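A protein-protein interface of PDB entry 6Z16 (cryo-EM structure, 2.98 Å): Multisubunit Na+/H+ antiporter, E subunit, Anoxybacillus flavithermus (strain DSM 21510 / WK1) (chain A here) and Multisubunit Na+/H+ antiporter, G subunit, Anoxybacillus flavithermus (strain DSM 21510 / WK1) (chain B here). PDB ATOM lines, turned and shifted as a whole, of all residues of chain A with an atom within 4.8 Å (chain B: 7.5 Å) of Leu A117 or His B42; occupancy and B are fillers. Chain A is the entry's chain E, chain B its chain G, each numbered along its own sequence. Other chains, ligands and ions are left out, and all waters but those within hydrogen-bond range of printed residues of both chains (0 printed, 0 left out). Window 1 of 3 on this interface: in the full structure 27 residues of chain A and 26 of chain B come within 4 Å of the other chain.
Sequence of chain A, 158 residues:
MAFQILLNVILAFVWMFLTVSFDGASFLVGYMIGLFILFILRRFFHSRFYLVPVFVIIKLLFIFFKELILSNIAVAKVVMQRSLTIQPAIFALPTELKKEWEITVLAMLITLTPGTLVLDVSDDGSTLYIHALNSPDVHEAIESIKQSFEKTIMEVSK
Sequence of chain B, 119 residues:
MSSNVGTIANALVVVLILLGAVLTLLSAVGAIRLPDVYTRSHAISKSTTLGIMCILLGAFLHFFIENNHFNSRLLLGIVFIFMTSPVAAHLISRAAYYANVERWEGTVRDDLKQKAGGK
A ring nitrogen (NE2) of His B42 lies within hydrogen-bond range of a ring nitrogen (ND1) of His A131 (3.1 Å).
The backbone carbonyl oxygen (O) of Leu A117 lies within hydrogen-bond range of the backbone NH (N) of His A131.
The backbone carbonyl oxygen (O) of Asp B36 sits at hydrogen-bond distance from the side-chain hydroxyl (OG1) of Thr B39 (3.0 Å).
The backbone carbonyl oxygen (O) of Ala B89 lies within hydrogen-bond range of the side-chain hydroxyl (OG) of Ser B93, at 2.9 Å.
The backbone carbonyl oxygen (O) of Gly A115 sits at hydrogen-bond distance from the backbone NH (N) of Leu A133, at 2.8 Å.
O of Ile A110 is in hydrogen-bond range of OG1 of Thr A116 (2.7 Å).
OG of Ser B93 lies within hydrogen-bond range of OG of Ser B41, at 3.1 Å.
Among the printed residues, pairs that only touch across the chains: Val A75 with Ala B43 (3.9 Å), Val A75 with Lys B46 (3.8 Å), Thr A111 with Lys B46 (3.9 Å), Thr A111 with Pro B86 (3.9 Å), Gly A115 with His B42 (3.8 Å), Thr A116 with His B42 (3.3 Å), Thr A116 with Lys B46 (3.7 Å), Leu A117 with Tyr B38 (3.98 Å), Leu A117 with Ser B41 (3.7 Å), Leu A117 with His B42 (3.5 Å), Leu A117 with Ser B93 (3.6 Å), Val A118 with His B90 (3.1 Å), His A131 with Tyr B38 (3.5 Å), Leu A133 with Thr B39 (3.7 Å) and Leu A133 with His B42 (3.8 Å).
Of the printed residues of chain B, Leu A117 touches Tyr B38, Ser B41, His B42 and Ser B93.
His B42 touches five residues of chain A.
Of the printed residues of chain A, Ser B93 touches Leu A117.
Of the printed residues of chain B, His A131 touches Tyr B38 and His B42.
Printed residues of chain A within 4 Å of Pro B86: Thr A111.
Of the printed residues of chain A, Ser B41 touches Leu A117.
The nearest printed residue of chain B that does not touch Leu A117 is Ala B89 (4.7 Å).
Hydrophobic or aromatic side chains of chain B that line the printed part of chain A: Tyr B38, His B42, Pro B86 and His B90.
Printed residues of chain A that touch a printed residue of chain B: Val A75, Thr A111, Gly A115, Thr A116, Leu A117, Val A118, His A131 and Leu A133.
Among the printed residues, no Asp or Glu carboxylate lies within 4 Å of a Lys or Arg side-chain nitrogen of the other chain.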
ATOM      1  N   VAL A  75     -21.873   2.203   8.991  1.00  0.00           N
ATOM      2  CA  VAL A  75     -20.503   2.103   8.485  1.00  0.00           C
ATOM      3  C   VAL A  75     -20.449   1.208   7.248  1.00  0.00           C
ATOM      4  O   VAL A  75     -19.687   1.482   6.309  1.00  0.00           O
ATOM      5  CB  VAL A  75     -19.567   1.624   9.615  1.00  0.00           C
ATOM      6  CG1 VAL A  75     -18.162   1.323   9.113  1.00  0.00           C
ATOM      7  CG2 VAL A  75     -19.480   2.686  10.692  1.00  0.00           C
ATOM      8  N   ILE A 110     -22.333   7.112  23.139  1.00  0.00           N
ATOM      9  CA  ILE A 110     -22.350   8.014  21.999  1.00  0.00           C
ATOM     10  C   ILE A 110     -21.174   7.757  21.060  1.00  0.00           C
ATOM     11  O   ILE A 110     -21.200   8.207  19.909  1.00  0.00           O
ATOM     12  CB  ILE A 110     -22.399   9.455  22.530  1.00  0.00           C
ATOM     13  CG1 ILE A 110     -22.915  10.435  21.493  1.00  0.00           C
ATOM     14  CG2 ILE A 110     -21.058   9.922  22.936  1.00  0.00           C
ATOM     15  CD1 ILE A 110     -23.145  11.786  22.092  1.00  0.00           C
ATOM     16  N   THR A 111     -20.150   7.027  21.512  1.00  0.00           N
ATOM     17  CA  THR A 111     -19.123   6.531  20.599  1.00  0.00           C
ATOM     18  C   THR A 111     -19.704   5.492  19.654  1.00  0.00           C
ATOM     19  O   THR A 111     -19.515   5.559  18.434  1.00  0.00           O
ATOM     20  CB  THR A 111     -17.965   5.920  21.393  1.00  0.00           C
ATOM     21  OG1 THR A 111     -17.351   6.919  22.210  1.00  0.00           O
ATOM     22  CG2 THR A 111     -16.924   5.313  20.465  1.00  0.00           C
ATOM     23  N   GLY A 115     -22.177   7.206  13.346  1.00  0.00           N
ATOM     24  CA  GLY A 115     -21.681   8.459  12.824  1.00  0.00           C
ATOM     25  C   GLY A 115     -20.991   9.377  13.808  1.00  0.00           C
ATOM     26  O   GLY A 115     -20.774  10.546  13.476  1.00  0.00           O
ATOM     27  N   THR A 116     -20.640   8.901  15.001  1.00  0.00           N
ATOM     28  CA  THR A 116     -20.063   9.755  16.031  1.00  0.00           C
ATOM     29  C   THR A 116     -18.903   9.059  16.727  1.00  0.00           C
ATOM     30  O   THR A 116     -18.808   7.831  16.749  1.00  0.00           O
ATOM     31  CB  THR A 116     -21.105  10.176  17.073  1.00  0.00           C
ATOM     32  OG1 THR A 116     -21.873   9.037  17.483  1.00  0.00           O
ATOM     33  CG2 THR A 116     -22.002  11.283  16.557  1.00  0.00           C
ATOM     34  N   LEU A 117     -18.024   9.876  17.309  1.00  0.00           N
ATOM     35  CA  LEU A 117     -16.820   9.413  17.986  1.00  0.00           C
ATOM     36  C   LEU A 117     -16.366  10.505  18.941  1.00  0.00           C
ATOM     37  O   LEU A 117     -16.278  11.667  18.545  1.00  0.00           O
ATOM     38  CB  LEU A 117     -15.707   9.106  16.987  1.00  0.00           C
ATOM     39  CG  LEU A 117     -14.405   8.518  17.519  1.00  0.00           C
ATOM     40  CD1 LEU A 117     -14.610   7.097  18.007  1.00  0.00           C
ATOM     41  CD2 LEU A 117     -13.340   8.588  16.454  1.00  0.00           C
ATOM     42  N   VAL A 118     -16.066  10.138  20.168  1.00  0.00           N
ATOM     43  CA  VAL A 118     -15.711  11.111  21.193  1.00  0.00           C
ATOM     44  C   VAL A 118     -14.224  11.409  21.109  1.00  0.00           C
ATOM     45  O   VAL A 118     -13.404  10.524  20.848  1.00  0.00           O
ATOM     46  CB  VAL A 118     -16.090  10.590  22.589  1.00  0.00           C
ATOM     47  CG1 VAL A 118     -15.876  11.645  23.677  1.00  0.00           C
ATOM     48  CG2 VAL A 118     -17.483  10.142  22.583  1.00  0.00           C
ATOM     49  N   LEU A 119     -13.888  12.677  21.290  1.00  0.00           N
ATOM     50  CA  LEU A 119     -12.551  13.118  21.639  1.00  0.00           C
ATOM     51  C   LEU A 119     -12.729  14.386  22.452  1.00  0.00           C
ATOM     52  O   LEU A 119     -13.595  15.196  22.124  1.00  0.00           O
ATOM     53  CB  LEU A 119     -11.696  13.337  20.384  1.00  0.00           C
ATOM     54  CG  LEU A 119     -12.207  14.213  19.233  1.00  0.00           C
ATOM     55  CD1 LEU A 119     -11.808  15.683  19.345  1.00  0.00           C
ATOM     56  CD2 LEU A 119     -11.768  13.629  17.903  1.00  0.00           C
ATOM     57  N   ILE A 130     -16.881  16.107  20.004  1.00  0.00           N
ATOM     58  CA  ILE A 130     -17.255  14.861  19.343  1.00  0.00           C
ATOM     59  C   ILE A 130     -17.099  15.031  17.837  1.00  0.00           C
ATOM     60  O   ILE A 130     -17.397  16.091  17.278  1.00  0.00           O
ATOM     61  CB  ILE A 130     -18.685  14.440  19.765  1.00  0.00           C
ATOM     62  CG1 ILE A 130     -19.144  13.138  19.110  1.00  0.00           C
ATOM     63  CG2 ILE A 130     -19.649  15.566  19.586  1.00  0.00           C
ATOM     64  CD1 ILE A 130     -20.321  12.545  19.798  1.00  0.00           C
ATOM     65  N   HIS A 131     -16.602  13.974  17.194  1.00  0.00           N
ATOM     66  CA  HIS A 131     -16.297  13.957  15.769  1.00  0.00           C
ATOM     67  C   HIS A 131     -17.415  13.241  15.016  1.00  0.00           C
ATOM     68  O   HIS A 131     -17.557  12.018  15.109  1.00  0.00           O
ATOM     69  CB  HIS A 131     -14.946  13.286  15.530  1.00  0.00           C
ATOM     70  CG  HIS A 131     -14.552  13.203  14.088  1.00  0.00           C
ATOM     71  ND1 HIS A 131     -14.905  12.142  13.283  1.00  0.00           N
ATOM     72  CD2 HIS A 131     -13.837  14.045  13.307  1.00  0.00           C
ATOM     73  CE1 HIS A 131     -14.426  12.336  12.069  1.00  0.00           C
ATOM     74  NE2 HIS A 131     -13.774  13.485  12.056  1.00  0.00           N
ATOM     75  N   ALA A 132     -18.190  14.007  14.257  1.00  0.00           N
ATOM     76  CA  ALA A 132     -19.227  13.455  13.403  1.00  0.00           C
ATOM     77  C   ALA A 132     -18.655  13.025  12.061  1.00  0.00           C
ATOM     78  O   ALA A 132     -17.903  13.766  11.420  1.00  0.00           O
ATOM     79  CB  ALA A 132     -20.335  14.480  13.177  1.00  0.00           C
ATOM     80  N   LEU A 133     -19.050  11.827  11.626  1.00  0.00           N
ATOM     81  CA  LEU A 133     -18.581  11.280  10.358  1.00  0.00           C
ATOM     82  C   LEU A 133     -19.255  11.953   9.167  1.00  0.00           C
ATOM     83  O   LEU A 133     -18.589  12.304   8.190  1.00  0.00           O
ATOM     84  CB  LEU A 133     -18.822   9.774  10.326  1.00  0.00           C
ATOM     85  CG  LEU A 133     -18.317   9.058   9.083  1.00  0.00           C
ATOM     86  CD1 LEU A 133     -16.834   9.261   8.966  1.00  0.00           C
ATOM     87  CD2 LEU A 133     -18.639   7.579   9.155  1.00  0.00           C
ATOM     88  N   SER B  27     -14.314  -3.930   7.974  1.00  0.00           N
ATOM     89  CA  SER B  27     -13.467  -3.059   8.789  1.00  0.00           C
ATOM     90  C   SER B  27     -12.105  -2.837   8.142  1.00  0.00           C
ATOM     91  O   SER B  27     -11.555  -1.733   8.195  1.00  0.00           O
ATOM     92  CB  SER B  27     -13.291  -3.650  10.184  1.00  0.00           C
ATOM     93  OG  SER B  27     -12.409  -2.861  10.956  1.00  0.00           O
ATOM     94  N   LEU B  34     -10.547   4.853   3.802  1.00  0.00           N
ATOM     95  CA  LEU B  34     -10.992   6.121   4.371  1.00  0.00           C
ATOM     96  C   LEU B  34      -9.809   7.070   4.574  1.00  0.00           C
ATOM     97  O   LEU B  34      -8.713   6.627   4.918  1.00  0.00           O
ATOM     98  CB  LEU B  34     -11.726   5.872   5.684  1.00  0.00           C
ATOM     99  CG  LEU B  34     -13.081   5.200   5.454  1.00  0.00           C
ATOM    100  CD1 LEU B  34     -13.726   4.806   6.757  1.00  0.00           C
ATOM    101  CD2 LEU B  34     -13.997   6.114   4.666  1.00  0.00           C
ATOM    102  N   ASP B  36      -8.861   9.803   6.567  1.00  0.00           N
ATOM    103  CA  ASP B  36      -8.418  10.503   7.760  1.00  0.00           C
ATOM    104  C   ASP B  36      -8.204   9.474   8.860  1.00  0.00           C
ATOM    105  O   ASP B  36      -8.669   8.339   8.756  1.00  0.00           O
ATOM    106  CB  ASP B  36      -9.463  11.548   8.169  1.00  0.00           C
ATOM    107  CG  ASP B  36      -8.924  12.590   9.106  1.00  0.00           C
ATOM    108  OD1 ASP B  36      -7.739  12.510   9.483  1.00  0.00           O
ATOM    109  OD2 ASP B  36      -9.702  13.499   9.457  1.00  0.00           O
ATOM    110  N   VAL B  37      -7.486   9.867   9.915  1.00  0.00           N
ATOM    111  CA  VAL B  37      -7.306   8.963  11.049  1.00  0.00           C
ATOM    112  C   VAL B  37      -8.629   8.744  11.788  1.00  0.00           C
ATOM    113  O   VAL B  37      -8.899   7.642  12.287  1.00  0.00           O
ATOM    114  CB  VAL B  37      -6.184   9.496  11.969  1.00  0.00           C
ATOM    115  CG1 VAL B  37      -6.494  10.894  12.488  1.00  0.00           C
ATOM    116  CG2 VAL B  37      -5.916   8.548  13.130  1.00  0.00           C
ATOM    117  N   TYR B  38      -9.511   9.744  11.791  1.00  0.00           N
ATOM    118  CA  TYR B  38     -10.723   9.669  12.595  1.00  0.00           C
ATOM    119  C   TYR B  38     -11.796   8.826  11.916  1.00  0.00           C
ATOM    120  O   TYR B  38     -12.525   8.084  12.586  1.00  0.00           O
ATOM    121  CB  TYR B  38     -11.235  11.077  12.854  1.00  0.00           C
ATOM    122  CG  TYR B  38     -10.185  11.989  13.415  1.00  0.00           C
ATOM    123  CD1 TYR B  38      -9.794  11.901  14.738  1.00  0.00           C
ATOM    124  CD2 TYR B  38      -9.592  12.953  12.617  1.00  0.00           C
ATOM    125  CE1 TYR B  38      -8.830  12.747  15.249  1.00  0.00           C
ATOM    126  CE2 TYR B  38      -8.633  13.802  13.120  1.00  0.00           C
ATOM    127  CZ  TYR B  38      -8.256  13.694  14.435  1.00  0.00           C
ATOM    128  OH  TYR B  38      -7.301  14.538  14.934  1.00  0.00           O
ATOM    129  N   THR B  39     -11.900   8.926  10.590  1.00  0.00           N
ATOM    130  CA  THR B  39     -12.818   8.078   9.842  1.00  0.00           C
ATOM    131  C   THR B  39     -12.411   6.615   9.933  1.00  0.00           C
ATOM    132  O   THR B  39     -13.263   5.721  10.051  1.00  0.00           O
ATOM    133  CB  THR B  39     -12.852   8.536   8.390  1.00  0.00           C
ATOM    134  OG1 THR B  39     -11.544   8.395   7.834  1.00  0.00           O
ATOM    135  CG2 THR B  39     -13.245   9.993   8.316  1.00  0.00           C
ATOM    136  N   ARG B  40     -11.102   6.355   9.897  1.00  0.00           N
ATOM    137  CA  ARG B  40     -10.603   5.007  10.120  1.00  0.00           C
ATOM    138  C   ARG B  40     -10.873   4.546  11.542  1.00  0.00           C
ATOM    139  O   ARG B  40     -11.114   3.356  11.757  1.00  0.00           O
ATOM    140  CB  ARG B  40      -9.112   4.951   9.810  1.00  0.00           C
ATOM    141  CG  ARG B  40      -8.799   5.130   8.347  1.00  0.00           C
ATOM    142  CD  ARG B  40      -7.324   5.388   8.136  1.00  0.00           C
ATOM    143  NE  ARG B  40      -7.058   5.802   6.762  1.00  0.00           N
ATOM    144  CZ  ARG B  40      -5.929   6.372   6.365  1.00  0.00           C
ATOM    145  NH1 ARG B  40      -4.972   6.624   7.238  1.00  0.00           N
ATOM    146  NH2 ARG B  40      -5.774   6.719   5.094  1.00  0.00           N
ATOM    147  N   SER B  41     -10.859   5.467  12.512  1.00  0.00           N
ATOM    148  CA  SER B  41     -11.207   5.114  13.887  1.00  0.00           C
ATOM    149  C   SER B  41     -12.655   4.646  13.987  1.00  0.00           C
ATOM    150  O   SER B  41     -12.928   3.604  14.599  1.00  0.00           O
ATOM    151  CB  SER B  41     -10.964   6.304  14.810  1.00  0.00           C
ATOM    152  OG  SER B  41      -9.605   6.690  14.805  1.00  0.00           O
ATOM    153  N   HIS B  42     -13.581   5.406  13.374  1.00  0.00           N
ATOM    154  CA  HIS B  42     -14.983   5.002  13.198  1.00  0.00           C
ATOM    155  C   HIS B  42     -15.107   3.582  12.668  1.00  0.00           C
ATOM    156  O   HIS B  42     -15.663   2.691  13.338  1.00  0.00           O
ATOM    157  CB  HIS B  42     -15.700   5.929  12.211  1.00  0.00           C
ATOM    158  CG  HIS B  42     -16.052   7.278  12.745  1.00  0.00           C
ATOM    159  ND1 HIS B  42     -17.104   7.482  13.606  1.00  0.00           N
ATOM    160  CD2 HIS B  42     -15.542   8.503  12.480  1.00  0.00           C
ATOM    161  CE1 HIS B  42     -17.206   8.770  13.877  1.00  0.00           C
ATOM    162  NE2 HIS B  42     -16.263   9.410  13.213  1.00  0.00           N
ATOM    163  N   ALA B  43     -14.547   3.367  11.470  1.00  0.00           N
ATOM    164  CA  ALA B  43     -14.728   2.109  10.746  1.00  0.00           C
ATOM    165  C   ALA B  43     -14.135   0.941  11.509  1.00  0.00           C
ATOM    166  O   ALA B  43     -14.832  -0.050  11.778  1.00  0.00           O
ATOM    167  CB  ALA B  43     -14.094   2.201   9.363  1.00  0.00           C
ATOM    168  N   ILE B  44     -12.868   1.076  11.920  1.00  0.00           N
ATOM    169  CA  ILE B  44     -12.150  -0.005  12.588  1.00  0.00           C
ATOM    170  C   ILE B  44     -12.814  -0.356  13.907  1.00  0.00           C
ATOM    171  O   ILE B  44     -13.209  -1.510  14.108  1.00  0.00           O
ATOM    172  CB  ILE B  44     -10.669   0.362  12.780  1.00  0.00           C
ATOM    173  CG1 ILE B  44      -9.944   0.355  11.438  1.00  0.00           C
ATOM    174  CG2 ILE B  44     -10.015  -0.609  13.720  1.00  0.00           C
ATOM    175  CD1 ILE B  44      -8.578   0.966  11.489  1.00  0.00           C
ATOM    176  N   SER B  45     -13.008   0.646  14.787  1.00  0.00           N
ATOM    177  CA  SER B  45     -13.647   0.502  16.091  1.00  0.00           C
ATOM    178  C   SER B  45     -14.964  -0.255  16.039  1.00  0.00           C
ATOM    179  O   SER B  45     -15.031  -1.413  16.491  1.00  0.00           O
ATOM    180  CB  SER B  45     -13.892   1.891  16.679  1.00  0.00           C
ATOM    181  OG  SER B  45     -14.637   1.827  17.878  1.00  0.00           O
ATOM    182  N   LYS B  46     -15.958   0.325  15.357  1.00  0.00           N
ATOM    183  CA  LYS B  46     -17.292  -0.255  15.419  1.00  0.00           C
ATOM    184  C   LYS B  46     -17.374  -1.567  14.645  1.00  0.00           C
ATOM    185  O   LYS B  46     -17.915  -2.564  15.162  1.00  0.00           O
ATOM    186  CB  LYS B  46     -18.318   0.763  14.927  1.00  0.00           C
ATOM    187  CG  LYS B  46     -18.364   1.984  15.832  1.00  0.00           C
ATOM    188  CD  LYS B  46     -19.508   2.916  15.512  1.00  0.00           C
ATOM    189  CE  LYS B  46     -19.267   3.777  14.299  1.00  0.00           C
ATOM    190  NZ  LYS B  46     -18.275   4.837  14.591  1.00  0.00           N
ATOM    191  N   SER B  47     -16.779  -1.623  13.445  1.00  0.00           N
ATOM    192  CA  SER B  47     -16.985  -2.801  12.621  1.00  0.00           C
ATOM    193  C   SER B  47     -16.192  -4.001  13.115  1.00  0.00           C
ATOM    194  O   SER B  47     -16.741  -5.108  13.158  1.00  0.00           O
ATOM    195  CB  SER B  47     -16.646  -2.497  11.168  1.00  0.00           C
ATOM    196  OG  SER B  47     -16.853  -3.652  10.374  1.00  0.00           O
ATOM    197  N   THR B  48     -14.922  -3.835  13.519  1.00  0.00           N
ATOM    198  CA  THR B  48     -14.231  -5.028  13.985  1.00  0.00           C
ATOM    199  C   THR B  48     -14.666  -5.418  15.391  1.00  0.00           C
ATOM    200  O   THR B  48     -14.576  -6.606  15.717  1.00  0.00           O
ATOM    201  CB  THR B  48     -12.698  -4.889  13.905  1.00  0.00           C
ATOM    202  OG1 THR B  48     -12.133  -6.196  13.766  1.00  0.00           O
ATOM    203  CG2 THR B  48     -12.093  -4.308  15.176  1.00  0.00           C
ATOM    204  N   PRO B  86     -13.876   0.350  21.885  1.00  0.00           N
ATOM    205  CA  PRO B  86     -14.158   1.763  21.584  1.00  0.00           C
ATOM    206  C   PRO B  86     -13.434   2.749  22.481  1.00  0.00           C
ATOM    207  O   PRO B  86     -13.144   3.862  22.029  1.00  0.00           O
ATOM    208  CB  PRO B  86     -15.677   1.869  21.758  1.00  0.00           C
ATOM    209  CG  PRO B  86     -16.165   0.526  21.582  1.00  0.00           C
ATOM    210  CD  PRO B  86     -15.144  -0.333  22.209  1.00  0.00           C
ATOM    211  N   ALA B  89     -10.168   3.142  20.771  1.00  0.00           N
ATOM    212  CA  ALA B  89     -10.280   4.071  19.648  1.00  0.00           C
ATOM    213  C   ALA B  89     -10.391   5.517  20.117  1.00  0.00           C
ATOM    214  O   ALA B  89      -9.822   6.420  19.495  1.00  0.00           O
ATOM    215  CB  ALA B  89     -11.477   3.703  18.783  1.00  0.00           C
ATOM    216  N   HIS B  90     -11.104   5.744  21.227  1.00  0.00           N
ATOM    217  CA  HIS B  90     -11.183   7.067  21.840  1.00  0.00           C
ATOM    218  C   HIS B  90      -9.815   7.583  22.264  1.00  0.00           C
ATOM    219  O   HIS B  90      -9.491   8.756  22.039  1.00  0.00           O
ATOM    220  CB  HIS B  90     -12.115   7.025  23.050  1.00  0.00           C
ATOM    221  CG  HIS B  90     -12.140   8.299  23.835  1.00  0.00           C
ATOM    222  ND1 HIS B  90     -11.282   8.543  24.885  1.00  0.00           N
ATOM    223  CD2 HIS B  90     -12.905   9.407  23.714  1.00  0.00           C
ATOM    224  CE1 HIS B  90     -11.524   9.742  25.382  1.00  0.00           C
ATOM    225  NE2 HIS B  90     -12.504  10.287  24.688  1.00  0.00           N
ATOM    226  N   LEU B  91      -9.003   6.723  22.878  1.00  0.00           N
ATOM    227  CA  LEU B  91      -7.694   7.160  23.354  1.00  0.00           C
ATOM    228  C   LEU B  91      -6.741   7.453  22.205  1.00  0.00           C
ATOM    229  O   LEU B  91      -6.011   8.452  22.247  1.00  0.00           O
ATOM    230  CB  LEU B  91      -7.110   6.115  24.298  1.00  0.00           C
ATOM    231  CG  LEU B  91      -7.810   6.116  25.651  1.00  0.00           C
ATOM    232  CD1 LEU B  91      -7.404   4.914  26.442  1.00  0.00           C
ATOM    233  CD2 LEU B  91      -7.467   7.389  26.409  1.00  0.00           C
ATOM    234  N   SER B  93      -7.657   8.388  19.215  1.00  0.00           N
ATOM    235  CA  SER B  93      -8.145   9.574  18.523  1.00  0.00           C
ATOM    236  C   SER B  93      -7.843  10.848  19.301  1.00  0.00           C
ATOM    237  O   SER B  93      -7.515  11.877  18.699  1.00  0.00           O
ATOM    238  CB  SER B  93      -9.639   9.443  18.258  1.00  0.00           C
ATOM    239  OG  SER B  93      -9.891   8.370  17.370  1.00  0.00           O
ATOM    240  N   ARG B  94      -7.913  10.803  20.636  1.00  0.00           N
ATOM    241  CA  ARG B  94      -7.511  11.976  21.410  1.00  0.00           C
ATOM    242  C   ARG B  94      -6.007  12.199  21.321  1.00  0.00           C
ATOM    243  O   ARG B  94      -5.544  13.349  21.269  1.00  0.00           O
ATOM    244  CB  ARG B  94      -7.938  11.849  22.873  1.00  0.00           C
ATOM    245  CG  ARG B  94      -7.764  13.167  23.618  1.00  0.00           C
ATOM    246  CD  ARG B  94      -8.167  13.162  25.086  1.00  0.00           C
ATOM    247  NE  ARG B  94      -7.265  12.383  25.923  1.00  0.00           N
ATOM    248  CZ  ARG B  94      -7.642  11.346  26.657  1.00  0.00           C
ATOM    249  NH1 ARG B  94      -8.913  10.979  26.675  1.00  0.00           N
ATOM    250  NH2 ARG B  94      -6.756  10.690  27.391  1.00  0.00           N
